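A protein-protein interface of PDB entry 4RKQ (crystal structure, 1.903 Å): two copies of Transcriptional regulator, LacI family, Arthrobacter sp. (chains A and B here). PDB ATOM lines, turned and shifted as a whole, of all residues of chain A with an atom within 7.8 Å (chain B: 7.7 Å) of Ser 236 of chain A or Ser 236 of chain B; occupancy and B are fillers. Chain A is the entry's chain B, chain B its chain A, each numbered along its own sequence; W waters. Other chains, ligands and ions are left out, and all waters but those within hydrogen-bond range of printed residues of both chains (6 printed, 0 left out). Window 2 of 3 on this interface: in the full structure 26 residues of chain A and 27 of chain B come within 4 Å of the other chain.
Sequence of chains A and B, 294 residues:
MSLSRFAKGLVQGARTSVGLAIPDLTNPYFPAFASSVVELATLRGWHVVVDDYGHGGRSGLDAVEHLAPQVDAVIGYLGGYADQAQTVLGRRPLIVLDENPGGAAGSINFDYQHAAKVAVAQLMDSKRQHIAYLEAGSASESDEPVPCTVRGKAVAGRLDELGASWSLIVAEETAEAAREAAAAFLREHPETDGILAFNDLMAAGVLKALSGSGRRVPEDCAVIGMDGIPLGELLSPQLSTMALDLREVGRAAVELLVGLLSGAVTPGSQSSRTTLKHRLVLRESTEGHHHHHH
The side-chain amino group (NZ) of Lys 208 of chain A is in hydrogen-bond range of the backbone carbonyl oxygen (O) of Leu 235 of chain B.
The side-chain amino group (NZ) of Lys 208 of chain B lies within hydrogen-bond range of the backbone carbonyl oxygen (O) of Leu 235 of chain A, at 2.7 Å.
The backbone carbonyl oxygen of Gln 238 of chain B lies within hydrogen-bond range of the backbone NH of Glu 284 of chain B, at 2.9 Å.
O of Gln 238 of chain A sits at hydrogen-bond distance from N of Ser 285 of chain A, 3.0 Å away.
The backbone NH (N) of Ser 285 of chain B is in hydrogen-bond range of the backbone carbonyl oxygen (O) of Gln 238 of chain B (3.0 Å).
OE1 of Glu 284 of chain A is in hydrogen-bond range of N of Gln 238 of chain A (3.0 Å).
Among the printed residues, pairs that only touch across the chains: Lys 208 of chain A with Glu 233 of chain B (3.4 Å), Glu 233 of chain A with Lys 208 of chain B (3.4 Å), Leu 234 of chain A with Leu 235 of chain B (3.4 Å), Leu 231 of chain A with Leu 231 of chain B (3.4 Å), Ser 236 of chain A with Ser 236 of chain B (3.6 Å), Leu 234 of chain A with Lys 208 of chain B (3.6 Å), Leu 235 of chain A with Leu 234 of chain B (3.6 Å), Lys 208 of chain A with Leu 234 of chain B (3.7 Å), Lys 208 of chain A with Ser 236 of chain B (3.7 Å), Lys 208 of chain A with Gln 238 of chain B (3.7 Å), Gln 238 of chain A with Lys 208 of chain B (3.8 Å) and Ser 236 of chain A with Lys 208 of chain B (3.96 Å).
Of the printed residues of chain B, Ser 236 of chain A touches Lys 208 and Ser 236.
Of the printed residues of chain A, Ser 236 of chain B touches Lys 208 (3.7 Å) and Ser 236 (3.6 Å).
No residue of chain B comes within 4 Å of Pro 237 of chain A.
No residue of chain A comes within 4 Å of Pro 237 of chain B.
Of the printed residues of chain B, Leu 234 of chain A touches Lys 208 and Leu 235.
Of the printed residues of chain B, Glu 233 of chain A touches Lys 208.
The nearest printed residue of chain A that does not touch Ser 236 of chain B is Ser 211 of chain A (5.0 Å).
The nearest printed residue of chain B that does not touch Gln 238 of chain A is Ser 211 of chain B (8.1 Å).
Of the 15 printed residues of chain B, 7 touch a printed residue of chain A.
Printed residues of chain B that touch a printed residue of chain A: Lys 208, Leu 231, Glu 233, Leu 234, Leu 235, Ser 236 and Gln 238.
Hydrophobic or aromatic side chains of chain A within 4 Å of the printed part of chain B: Leu 231 and Leu 235.
Among the printed residues, 14 pairs touch across the chains.
Among the printed residues, no Asp or Glu carboxylate lies within 4 Å of a Lys or Arg side-chain nitrogen of the other chain.
Lys 208 of chain A touches Leu 234 of chain B, and with the chains exchanged Leu 234 of chain A touches Lys 208 of chain B.
Lys 208 of chain A touches Ser 236 of chain B, and with the chains exchanged Ser 236 of chain A touches Lys 208 of chain B.
Lys 208 of chain A touches Gln 238 of chain B, and with the chains exchanged Gln 238 of chain A touches Lys 208 of chain B.
Leu 231 of chain B touches its own counterpart, Leu 231 of chain A.
15 positions are printed for both chains.
Of the 14 pairs that touch across the chains among the printed residues, 14 have their exchanged pair printed and touching as well.
Water W6 lies within hydrogen-bond range of OG of Ser 236 of chain B (2.5 Å), OE1 of Glu 284 of chain B (2.7 Å) and NZ of Lys 208 of chain A (3.2 Å).
Water W4 lies within hydrogen-bond range of the side-chain hydroxyl of Ser 236 of chain A, the side-chain carboxylate of Glu 284 of chain A and the side-chain amino group of Lys 208 of chain B.
Water W2 lies within hydrogen-bond range of O of Leu 234 of chain A (2.8 Å), N of Ser 236 of chain B (3.0 Å) and N of Ser 236 of chain A (3.2 Å).
Water W5 lies within hydrogen-bond range of O of Leu 234 of chain B (2.8 Å), N of Ser 236 of chain A (3.0 Å) and N of Ser 236 of chain B (3.3 Å).
Water W1 lies within hydrogen-bond range of OE1 of Gln 238 of chain B (2.9 Å), NZ of Lys 208 of chain A (2.9 Å) and OE2 of Glu 284 of chain B (3.0 Å).
Water W3 lies within hydrogen-bond range of the side-chain amino group of Lys 208 of chain B (2.9 Å), the side-chain amide oxygen of Gln 238 of chain A (3.0 Å) and the side-chain carboxylate of Glu 284 of chain A (3.3 Å).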
ATOM      1  N   LEU A 207     -30.713 -33.548   7.738  1.00  0.00           N
ATOM      2  CA  LEU A 207     -30.133 -33.199   9.036  1.00  0.00           C
ATOM      3  C   LEU A 207     -30.649 -31.858   9.532  1.00  0.00           C
ATOM      4  O   LEU A 207     -30.806 -31.661  10.729  1.00  0.00           O
ATOM      5  CB  LEU A 207     -28.605 -33.129   8.984  1.00  0.00           C
ATOM      6  CG  LEU A 207     -27.841 -34.432   8.828  1.00  0.00           C
ATOM      7  CD1 LEU A 207     -26.394 -34.137   8.485  1.00  0.00           C
ATOM      8  CD2 LEU A 207     -27.939 -35.285  10.064  1.00  0.00           C
ATOM      9  N   LYS A 208     -30.889 -30.939   8.602  1.00  0.00           N
ATOM     10  CA  LYS A 208     -31.390 -29.614   8.922  1.00  0.00           C
ATOM     11  C   LYS A 208     -32.856 -29.662   9.332  1.00  0.00           C
ATOM     12  O   LYS A 208     -33.265 -28.936  10.226  1.00  0.00           O
ATOM     13  CB  LYS A 208     -31.226 -28.684   7.702  1.00  0.00           C
ATOM     14  CG  LYS A 208     -30.846 -27.267   8.028  1.00  0.00           C
ATOM     15  CD  LYS A 208     -29.647 -27.315   8.946  1.00  0.00           C
ATOM     16  CE  LYS A 208     -28.657 -26.211   8.704  1.00  0.00           C
ATOM     17  NZ  LYS A 208     -27.895 -26.098   9.956  1.00  0.00           N
ATOM     18  N   SER A 211     -32.651 -31.184  12.964  1.00  0.00           N
ATOM     19  CA  SER A 211     -32.260 -30.060  13.847  1.00  0.00           C
ATOM     20  C   SER A 211     -33.373 -29.060  14.087  1.00  0.00           C
ATOM     21  O   SER A 211     -33.651 -28.659  15.235  1.00  0.00           O
ATOM     22  CB  SER A 211     -31.082 -29.307  13.213  1.00  0.00           C
ATOM     23  OG  SER A 211     -31.002 -28.000  13.709  1.00  0.00           O
ATOM     24  N   VAL A 217     -29.588 -36.056  16.896  1.00  0.00           N
ATOM     25  CA  VAL A 217     -29.068 -37.006  15.931  1.00  0.00           C
ATOM     26  C   VAL A 217     -27.755 -37.445  16.505  1.00  0.00           C
ATOM     27  O   VAL A 217     -26.891 -36.586  16.749  1.00  0.00           O
ATOM     28  CB  VAL A 217     -28.868 -36.353  14.534  1.00  0.00           C
ATOM     29  CG1 VAL A 217     -28.076 -37.305  13.622  1.00  0.00           C
ATOM     30  CG2 VAL A 217     -30.197 -36.035  13.860  1.00  0.00           C
ATOM     31  N   LEU A 231     -17.969 -32.457   1.984  1.00  0.00           N
ATOM     32  CA  LEU A 231     -18.960 -31.708   2.779  1.00  0.00           C
ATOM     33  C   LEU A 231     -19.416 -32.455   4.030  1.00  0.00           C
ATOM     34  O   LEU A 231     -19.683 -31.848   5.069  1.00  0.00           O
ATOM     35  CB  LEU A 231     -20.143 -31.417   1.821  1.00  0.00           C
ATOM     36  CG  LEU A 231     -21.473 -30.825   2.176  1.00  0.00           C
ATOM     37  CD1 LEU A 231     -22.340 -31.916   2.764  1.00  0.00           C
ATOM     38  CD2 LEU A 231     -21.281 -29.665   3.128  1.00  0.00           C
ATOM     39  N   GLY A 232     -19.550 -33.771   3.911  1.00  0.00           N
ATOM     40  CA  GLY A 232     -19.959 -34.612   5.013  1.00  0.00           C
ATOM     41  C   GLY A 232     -19.160 -34.450   6.286  1.00  0.00           C
ATOM     42  O   GLY A 232     -19.699 -34.631   7.368  1.00  0.00           O
ATOM     43  N   GLU A 233     -17.883 -34.086   6.154  1.00  0.00           N
ATOM     44  CA  GLU A 233     -16.966 -33.934   7.303  1.00  0.00           C
ATOM     45  C   GLU A 233     -17.118 -32.574   7.979  1.00  0.00           C
ATOM     46  O   GLU A 233     -16.592 -32.352   9.071  1.00  0.00           O
ATOM     47  CB  GLU A 233     -15.504 -34.196   6.860  1.00  0.00           C
ATOM     48  CG  GLU A 233     -15.300 -35.654   6.463  1.00  0.00           C
ATOM     49  CD  GLU A 233     -13.848 -36.048   6.216  1.00  0.00           C
ATOM     50  OE1 GLU A 233     -13.017 -35.158   5.985  1.00  0.00           O
ATOM     51  OE2 GLU A 233     -13.534 -37.261   6.244  1.00  0.00           O
ATOM     52  N   LEU A 234     -17.886 -31.691   7.353  1.00  0.00           N
ATOM     53  CA  LEU A 234     -18.024 -30.328   7.840  1.00  0.00           C
ATOM     54  C   LEU A 234     -19.349 -30.051   8.413  1.00  0.00           C
ATOM     55  O   LEU A 234     -19.543 -29.005   9.043  1.00  0.00           O
ATOM     56  CB  LEU A 234     -17.765 -29.352   6.703  1.00  0.00           C
ATOM     57  CG  LEU A 234     -16.351 -29.485   6.091  1.00  0.00           C
ATOM     58  CD1 LEU A 234     -16.245 -28.555   4.888  1.00  0.00           C
ATOM     59  CD2 LEU A 234     -15.237 -29.234   7.081  1.00  0.00           C
ATOM     60  N   LEU A 235     -20.303 -30.941   8.171  1.00  0.00           N
ATOM     61  CA  LEU A 235     -21.589 -30.818   8.832  1.00  0.00           C
ATOM     62  C   LEU A 235     -21.482 -31.126  10.320  1.00  0.00           C
ATOM     63  O   LEU A 235     -20.530 -31.766  10.774  1.00  0.00           O
ATOM     64  CB  LEU A 235     -22.617 -31.775   8.202  1.00  0.00           C
ATOM     65  CG  LEU A 235     -22.817 -31.651   6.682  1.00  0.00           C
ATOM     66  CD1 LEU A 235     -23.839 -32.633   6.136  1.00  0.00           C
ATOM     67  CD2 LEU A 235     -23.196 -30.255   6.271  1.00  0.00           C
ATOM     68  N   SER A 236     -22.510 -30.708  11.053  1.00  0.00           N
ATOM     69  CA  SER A 236     -22.628 -31.016  12.451  1.00  0.00           C
ATOM     70  C   SER A 236     -24.067 -31.446  12.719  1.00  0.00           C
ATOM     71  O   SER A 236     -24.988 -30.657  12.561  1.00  0.00           O
ATOM     72  CB  SER A 236     -22.277 -29.789  13.286  1.00  0.00           C
ATOM     73  OG  SER A 236     -22.142 -30.153  14.643  1.00  0.00           O
ATOM     74  N   PRO A 237     -24.285 -32.719  13.042  1.00  0.00           N
ATOM     75  CA  PRO A 237     -23.272 -33.766  13.036  1.00  0.00           C
ATOM     76  C   PRO A 237     -22.685 -34.145  11.687  1.00  0.00           C
ATOM     77  O   PRO A 237     -23.346 -34.059  10.668  1.00  0.00           O
ATOM     78  CB  PRO A 237     -24.055 -34.981  13.548  1.00  0.00           C
ATOM     79  CG  PRO A 237     -25.415 -34.740  13.006  1.00  0.00           C
ATOM     80  CD  PRO A 237     -25.642 -33.267  13.121  1.00  0.00           C
ATOM     81  N   GLN A 238     -21.456 -34.651  11.718  1.00  0.00           N
ATOM     82  CA  GLN A 238     -20.804 -35.152  10.561  1.00  0.00           C
ATOM     83  C   GLN A 238     -21.612 -36.328  10.023  1.00  0.00           C
ATOM     84  O   GLN A 238     -22.120 -37.133  10.776  1.00  0.00           O
ATOM     85  CB  GLN A 238     -19.366 -35.563  10.901  1.00  0.00           C
ATOM     86  CG  GLN A 238     -18.462 -34.358  11.194  1.00  0.00           C
ATOM     87  CD  GLN A 238     -17.000 -34.726  11.376  1.00  0.00           C
ATOM     88  OE1 GLN A 238     -16.288 -34.147  12.198  1.00  0.00           O
ATOM     89  NE2 GLN A 238     -16.547 -35.663  10.619  1.00  0.00           N
ATOM     90  N   LEU A 239     -21.698 -36.407   8.707  1.00  0.00           N
ATOM     91  CA  LEU A 239     -22.594 -37.345   7.999  1.00  0.00           C
ATOM     92  C   LEU A 239     -22.020 -38.744   7.805  1.00  0.00           C
ATOM     93  O   LEU A 239     -20.999 -38.953   7.117  1.00  0.00           O
ATOM     94  CB  LEU A 239     -22.929 -36.746   6.641  1.00  0.00           C
ATOM     95  CG  LEU A 239     -23.896 -37.504   5.751  1.00  0.00           C
ATOM     96  CD1 LEU A 239     -25.201 -37.708   6.495  1.00  0.00           C
ATOM     97  CD2 LEU A 239     -24.089 -36.818   4.391  1.00  0.00           C
ATOM     98  N   GLU A 284     -20.845 -39.040  12.795  1.00  0.00           N
ATOM     99  CA  GLU A 284     -21.586 -38.737  13.986  1.00  0.00           C
ATOM    100  C   GLU A 284     -23.090 -38.839  13.818  1.00  0.00           C
ATOM    101  O   GLU A 284     -23.805 -38.712  14.790  1.00  0.00           O
ATOM    102  CB  GLU A 284     -21.261 -37.319  14.430  1.00  0.00           C
ATOM    103  CG  GLU A 284     -19.798 -37.075  14.695  1.00  0.00           C
ATOM    104  CD  GLU A 284     -19.476 -35.605  14.973  1.00  0.00           C
ATOM    105  OE1 GLU A 284     -20.154 -34.681  14.475  1.00  0.00           O
ATOM    106  OE2 GLU A 284     -18.494 -35.373  15.696  1.00  0.00           O
ATOM    107  N   SER A 285     -23.589 -39.052  12.598  1.00  0.00           N
ATOM    108  CA  SER A 285     -25.026 -39.085  12.343  1.00  0.00           C
ATOM    109  C   SER A 285     -25.661 -40.474  12.506  1.00  0.00           C
ATOM    110  O   SER A 285     -26.853 -40.646  12.248  1.00  0.00           O
ATOM    111  CB  SER A 285     -25.359 -38.519  10.951  1.00  0.00           C
ATOM    112  OG  SER A 285     -24.994 -39.390   9.900  1.00  0.00           O
ATOM    113  N   LEU B 207     -15.474 -23.274  12.333  1.00  0.00           N
ATOM    114  CA  LEU B 207     -16.604 -23.753  13.113  1.00  0.00           C
ATOM    115  C   LEU B 207     -16.337 -25.062  13.776  1.00  0.00           C
ATOM    116  O   LEU B 207     -16.712 -25.230  14.942  1.00  0.00           O
ATOM    117  CB  LEU B 207     -17.876 -23.863  12.285  1.00  0.00           C
ATOM    118  CG  LEU B 207     -18.466 -22.553  11.776  1.00  0.00           C
ATOM    119  CD1 LEU B 207     -19.626 -22.898  10.870  1.00  0.00           C
ATOM    120  CD2 LEU B 207     -18.934 -21.649  12.907  1.00  0.00           C
ATOM    121  N   LYS B 208     -15.679 -25.988  13.063  1.00  0.00           N
ATOM    122  CA  LYS B 208     -15.313 -27.301  13.601  1.00  0.00           C
ATOM    123  C   LYS B 208     -14.293 -27.190  14.749  1.00  0.00           C
ATOM    124  O   LYS B 208     -14.361 -27.921  15.740  1.00  0.00           O
ATOM    125  CB  LYS B 208     -14.756 -28.205  12.477  1.00  0.00           C
ATOM    126  CG  LYS B 208     -15.118 -29.678  12.581  1.00  0.00           C
ATOM    127  CD  LYS B 208     -16.205 -30.078  11.581  1.00  0.00           C
ATOM    128  CE  LYS B 208     -17.603 -29.618  11.988  1.00  0.00           C
ATOM    129  NZ  LYS B 208     -18.541 -30.720  12.352  1.00  0.00           N
ATOM    130  N   SER B 211     -16.186 -25.896  17.770  1.00  0.00           N
ATOM    131  CA  SER B 211     -17.047 -26.970  18.304  1.00  0.00           C
ATOM    132  C   SER B 211     -16.168 -27.997  19.063  1.00  0.00           C
ATOM    133  O   SER B 211     -16.437 -28.346  20.199  1.00  0.00           O
ATOM    134  CB  SER B 211     -17.809 -27.633  17.146  1.00  0.00           C
ATOM    135  OG  SER B 211     -18.732 -28.609  17.599  1.00  0.00           O
ATOM    136  N   VAL B 217     -21.043 -21.222  19.222  1.00  0.00           N
ATOM    137  CA  VAL B 217     -21.101 -20.210  18.199  1.00  0.00           C
ATOM    138  C   VAL B 217     -22.539 -19.953  17.911  1.00  0.00           C
ATOM    139  O   VAL B 217     -23.242 -20.882  17.520  1.00  0.00           O
ATOM    140  CB  VAL B 217     -20.424 -20.690  16.907  1.00  0.00           C
ATOM    141  CG1 VAL B 217     -20.614 -19.648  15.822  1.00  0.00           C
ATOM    142  CG2 VAL B 217     -18.986 -21.017  17.179  1.00  0.00           C
ATOM    143  N   LEU B 231     -23.070 -24.138   0.724  1.00  0.00           N
ATOM    144  CA  LEU B 231     -22.656 -24.899   1.919  1.00  0.00           C
ATOM    145  C   LEU B 231     -22.977 -24.142   3.251  1.00  0.00           C
ATOM    146  O   LEU B 231     -23.226 -24.756   4.292  1.00  0.00           O
ATOM    147  CB  LEU B 231     -21.140 -25.112   1.828  1.00  0.00           C
ATOM    148  CG  LEU B 231     -20.398 -26.217   2.567  1.00  0.00           C
ATOM    149  CD1 LEU B 231     -18.909 -25.951   2.531  1.00  0.00           C
ATOM    150  CD2 LEU B 231     -20.828 -26.372   3.996  1.00  0.00           C
ATOM    151  N   GLY B 232     -22.916 -22.820   3.214  1.00  0.00           N
ATOM    152  CA  GLY B 232     -23.112 -21.999   4.398  1.00  0.00           C
ATOM    153  C   GLY B 232     -24.491 -22.219   5.004  1.00  0.00           C
ATOM    154  O   GLY B 232     -24.646 -22.096   6.196  1.00  0.00           O
ATOM    155  N   GLU B 233     -25.478 -22.567   4.184  1.00  0.00           N
ATOM    156  CA  GLU B 233     -26.827 -22.795   4.675  1.00  0.00           C
ATOM    157  C   GLU B 233     -26.988 -24.182   5.269  1.00  0.00           C
ATOM    158  O   GLU B 233     -27.973 -24.443   5.925  1.00  0.00           O
ATOM    159  CB  GLU B 233     -27.836 -22.590   3.540  1.00  0.00           C
ATOM    160  CG  GLU B 233     -27.977 -21.123   3.148  1.00  0.00           C
ATOM    161  CD  GLU B 233     -28.928 -20.874   1.980  1.00  0.00           C
ATOM    162  OE1 GLU B 233     -29.753 -21.753   1.643  1.00  0.00           O
ATOM    163  OE2 GLU B 233     -28.844 -19.777   1.397  1.00  0.00           O
ATOM    164  N   LEU B 234     -26.024 -25.072   5.019  1.00  0.00           N
ATOM    165  CA  LEU B 234     -26.085 -26.467   5.483  1.00  0.00           C
ATOM    166  C   LEU B 234     -25.274 -26.731   6.747  1.00  0.00           C
ATOM    167  O   LEU B 234     -25.506 -27.706   7.436  1.00  0.00           O
ATOM    168  CB  LEU B 234     -25.600 -27.410   4.373  1.00  0.00           C
ATOM    169  CG  LEU B 234     -26.391 -27.217   3.052  1.00  0.00           C
ATOM    170  CD1 LEU B 234     -25.910 -28.185   1.998  1.00  0.00           C
ATOM    171  CD2 LEU B 234     -27.879 -27.387   3.260  1.00  0.00           C
ATOM    172  N   LEU B 235     -24.283 -25.891   7.010  1.00  0.00           N
ATOM    173  CA  LEU B 235     -23.530 -25.946   8.251  1.00  0.00           C
ATOM    174  C   LEU B 235     -24.426 -25.682   9.462  1.00  0.00           C
ATOM    175  O   LEU B 235     -25.493 -25.084   9.339  1.00  0.00           O
ATOM    176  CB  LEU B 235     -22.413 -24.927   8.249  1.00  0.00           C
ATOM    177  CG  LEU B 235     -21.398 -25.073   7.107  1.00  0.00           C
ATOM    178  CD1 LEU B 235     -20.398 -23.938   7.101  1.00  0.00           C
ATOM    179  CD2 LEU B 235     -20.657 -26.383   7.170  1.00  0.00           C
ATOM    180  N   SER B 236     -23.984 -26.175  10.609  1.00  0.00           N
ATOM    181  CA  SER B 236     -24.621 -25.866  11.885  1.00  0.00           C
ATOM    182  C   SER B 236     -23.558 -25.381  12.862  1.00  0.00           C
ATOM    183  O   SER B 236     -22.659 -26.141  13.211  1.00  0.00           O
ATOM    184  CB  SER B 236     -25.327 -27.102  12.441  1.00  0.00           C
ATOM    185  OG  SER B 236     -26.210 -26.732  13.478  1.00  0.00           O
ATOM    186  N   PRO B 237     -23.624 -24.103  13.291  1.00  0.00           N
ATOM    187  CA  PRO B 237     -24.629 -23.110  12.871  1.00  0.00           C
ATOM    188  C   PRO B 237     -24.438 -22.681  11.428  1.00  0.00           C
ATOM    189  O   PRO B 237     -23.316 -22.809  10.902  1.00  0.00           O
ATOM    190  CB  PRO B 237     -24.329 -21.918  13.777  1.00  0.00           C
ATOM    191  CG  PRO B 237     -22.871 -22.033  14.050  1.00  0.00           C
ATOM    192  CD  PRO B 237     -22.546 -23.509  14.084  1.00  0.00           C
ATOM    193  N   GLN B 238     -25.505 -22.199  10.814  1.00  0.00           N
ATOM    194  CA  GLN B 238     -25.416 -21.674   9.481  1.00  0.00           C
ATOM    195  C   GLN B 238     -24.531 -20.433   9.493  1.00  0.00           C
ATOM    196  O   GLN B 238     -24.586 -19.604  10.407  1.00  0.00           O
ATOM    197  CB  GLN B 238     -26.789 -21.352   8.946  1.00  0.00           C
ATOM    198  CG  GLN B 238     -27.685 -22.560   8.780  1.00  0.00           C
ATOM    199  CD  GLN B 238     -29.016 -22.158   8.176  1.00  0.00           C
ATOM    200  OE1 GLN B 238     -30.069 -22.673   8.532  1.00  0.00           O
ATOM    201  NE2 GLN B 238     -28.967 -21.225   7.279  1.00  0.00           N
ATOM    202  N   LEU B 239     -23.734 -20.310   8.448  1.00  0.00           N
ATOM    203  CA  LEU B 239     -22.564 -19.447   8.449  1.00  0.00           C
ATOM    204  C   LEU B 239     -22.901 -18.070   7.968  1.00  0.00           C
ATOM    205  O   LEU B 239     -23.432 -17.888   6.867  1.00  0.00           O
ATOM    206  CB  LEU B 239     -21.456 -20.041   7.571  1.00  0.00           C
ATOM    207  CG  LEU B 239     -20.208 -19.201   7.325  1.00  0.00           C
ATOM    208  CD1 LEU B 239     -19.467 -18.930   8.601  1.00  0.00           C
ATOM    209  CD2 LEU B 239     -19.288 -19.904   6.341  1.00  0.00           C
ATOM    210  N   GLU B 284     -26.641 -17.887  11.387  1.00  0.00           N
ATOM    211  CA  GLU B 284     -26.609 -18.234  12.785  1.00  0.00           C
ATOM    212  C   GLU B 284     -25.290 -18.068  13.481  1.00  0.00           C
ATOM    213  O   GLU B 284     -25.239 -18.210  14.694  1.00  0.00           O
ATOM    214  CB  GLU B 284     -27.081 -19.687  12.980  1.00  0.00           C
ATOM    215  CG  GLU B 284     -28.476 -19.943  12.449  1.00  0.00           C
ATOM    216  CD  GLU B 284     -28.822 -21.420  12.424  1.00  0.00           C
ATOM    217  OE1 GLU B 284     -27.893 -22.269  12.412  1.00  0.00           O
ATOM    218  OE2 GLU B 284     -30.030 -21.728  12.437  1.00  0.00           O
ATOM    219  N   SER B 285     -24.198 -17.783  12.760  1.00  0.00           N
ATOM    220  CA  SER B 285     -22.880 -17.799  13.406  1.00  0.00           C
ATOM    221  C   SER B 285     -22.497 -16.414  13.929  1.00  0.00           C
ATOM    222  O   SER B 285     -21.398 -16.212  14.404  1.00  0.00           O
ATOM    223  CB  SER B 285     -21.797 -18.368  12.500  1.00  0.00           C
ATOM    224  OG  SER B 285     -21.598 -17.490  11.423  1.00  0.00           O
HETATM  225  O   HOH W   1     -29.942 -24.299  10.873  1.00  0.00           O
HETATM  226  O   HOH W   2     -21.392 -27.684  10.702  1.00  0.00           O
HETATM  227  O   HOH W   3     -17.463 -32.513  14.398  1.00  0.00           O
HETATM  228  O   HOH W   4     -20.268 -31.994  15.006  1.00  0.00           O
HETATM  229  O   HOH W   5     -24.817 -29.206   9.741  1.00  0.00           O
HETATM  230  O   HOH W   6     -27.827 -24.956  12.955  1.00  0.00           O
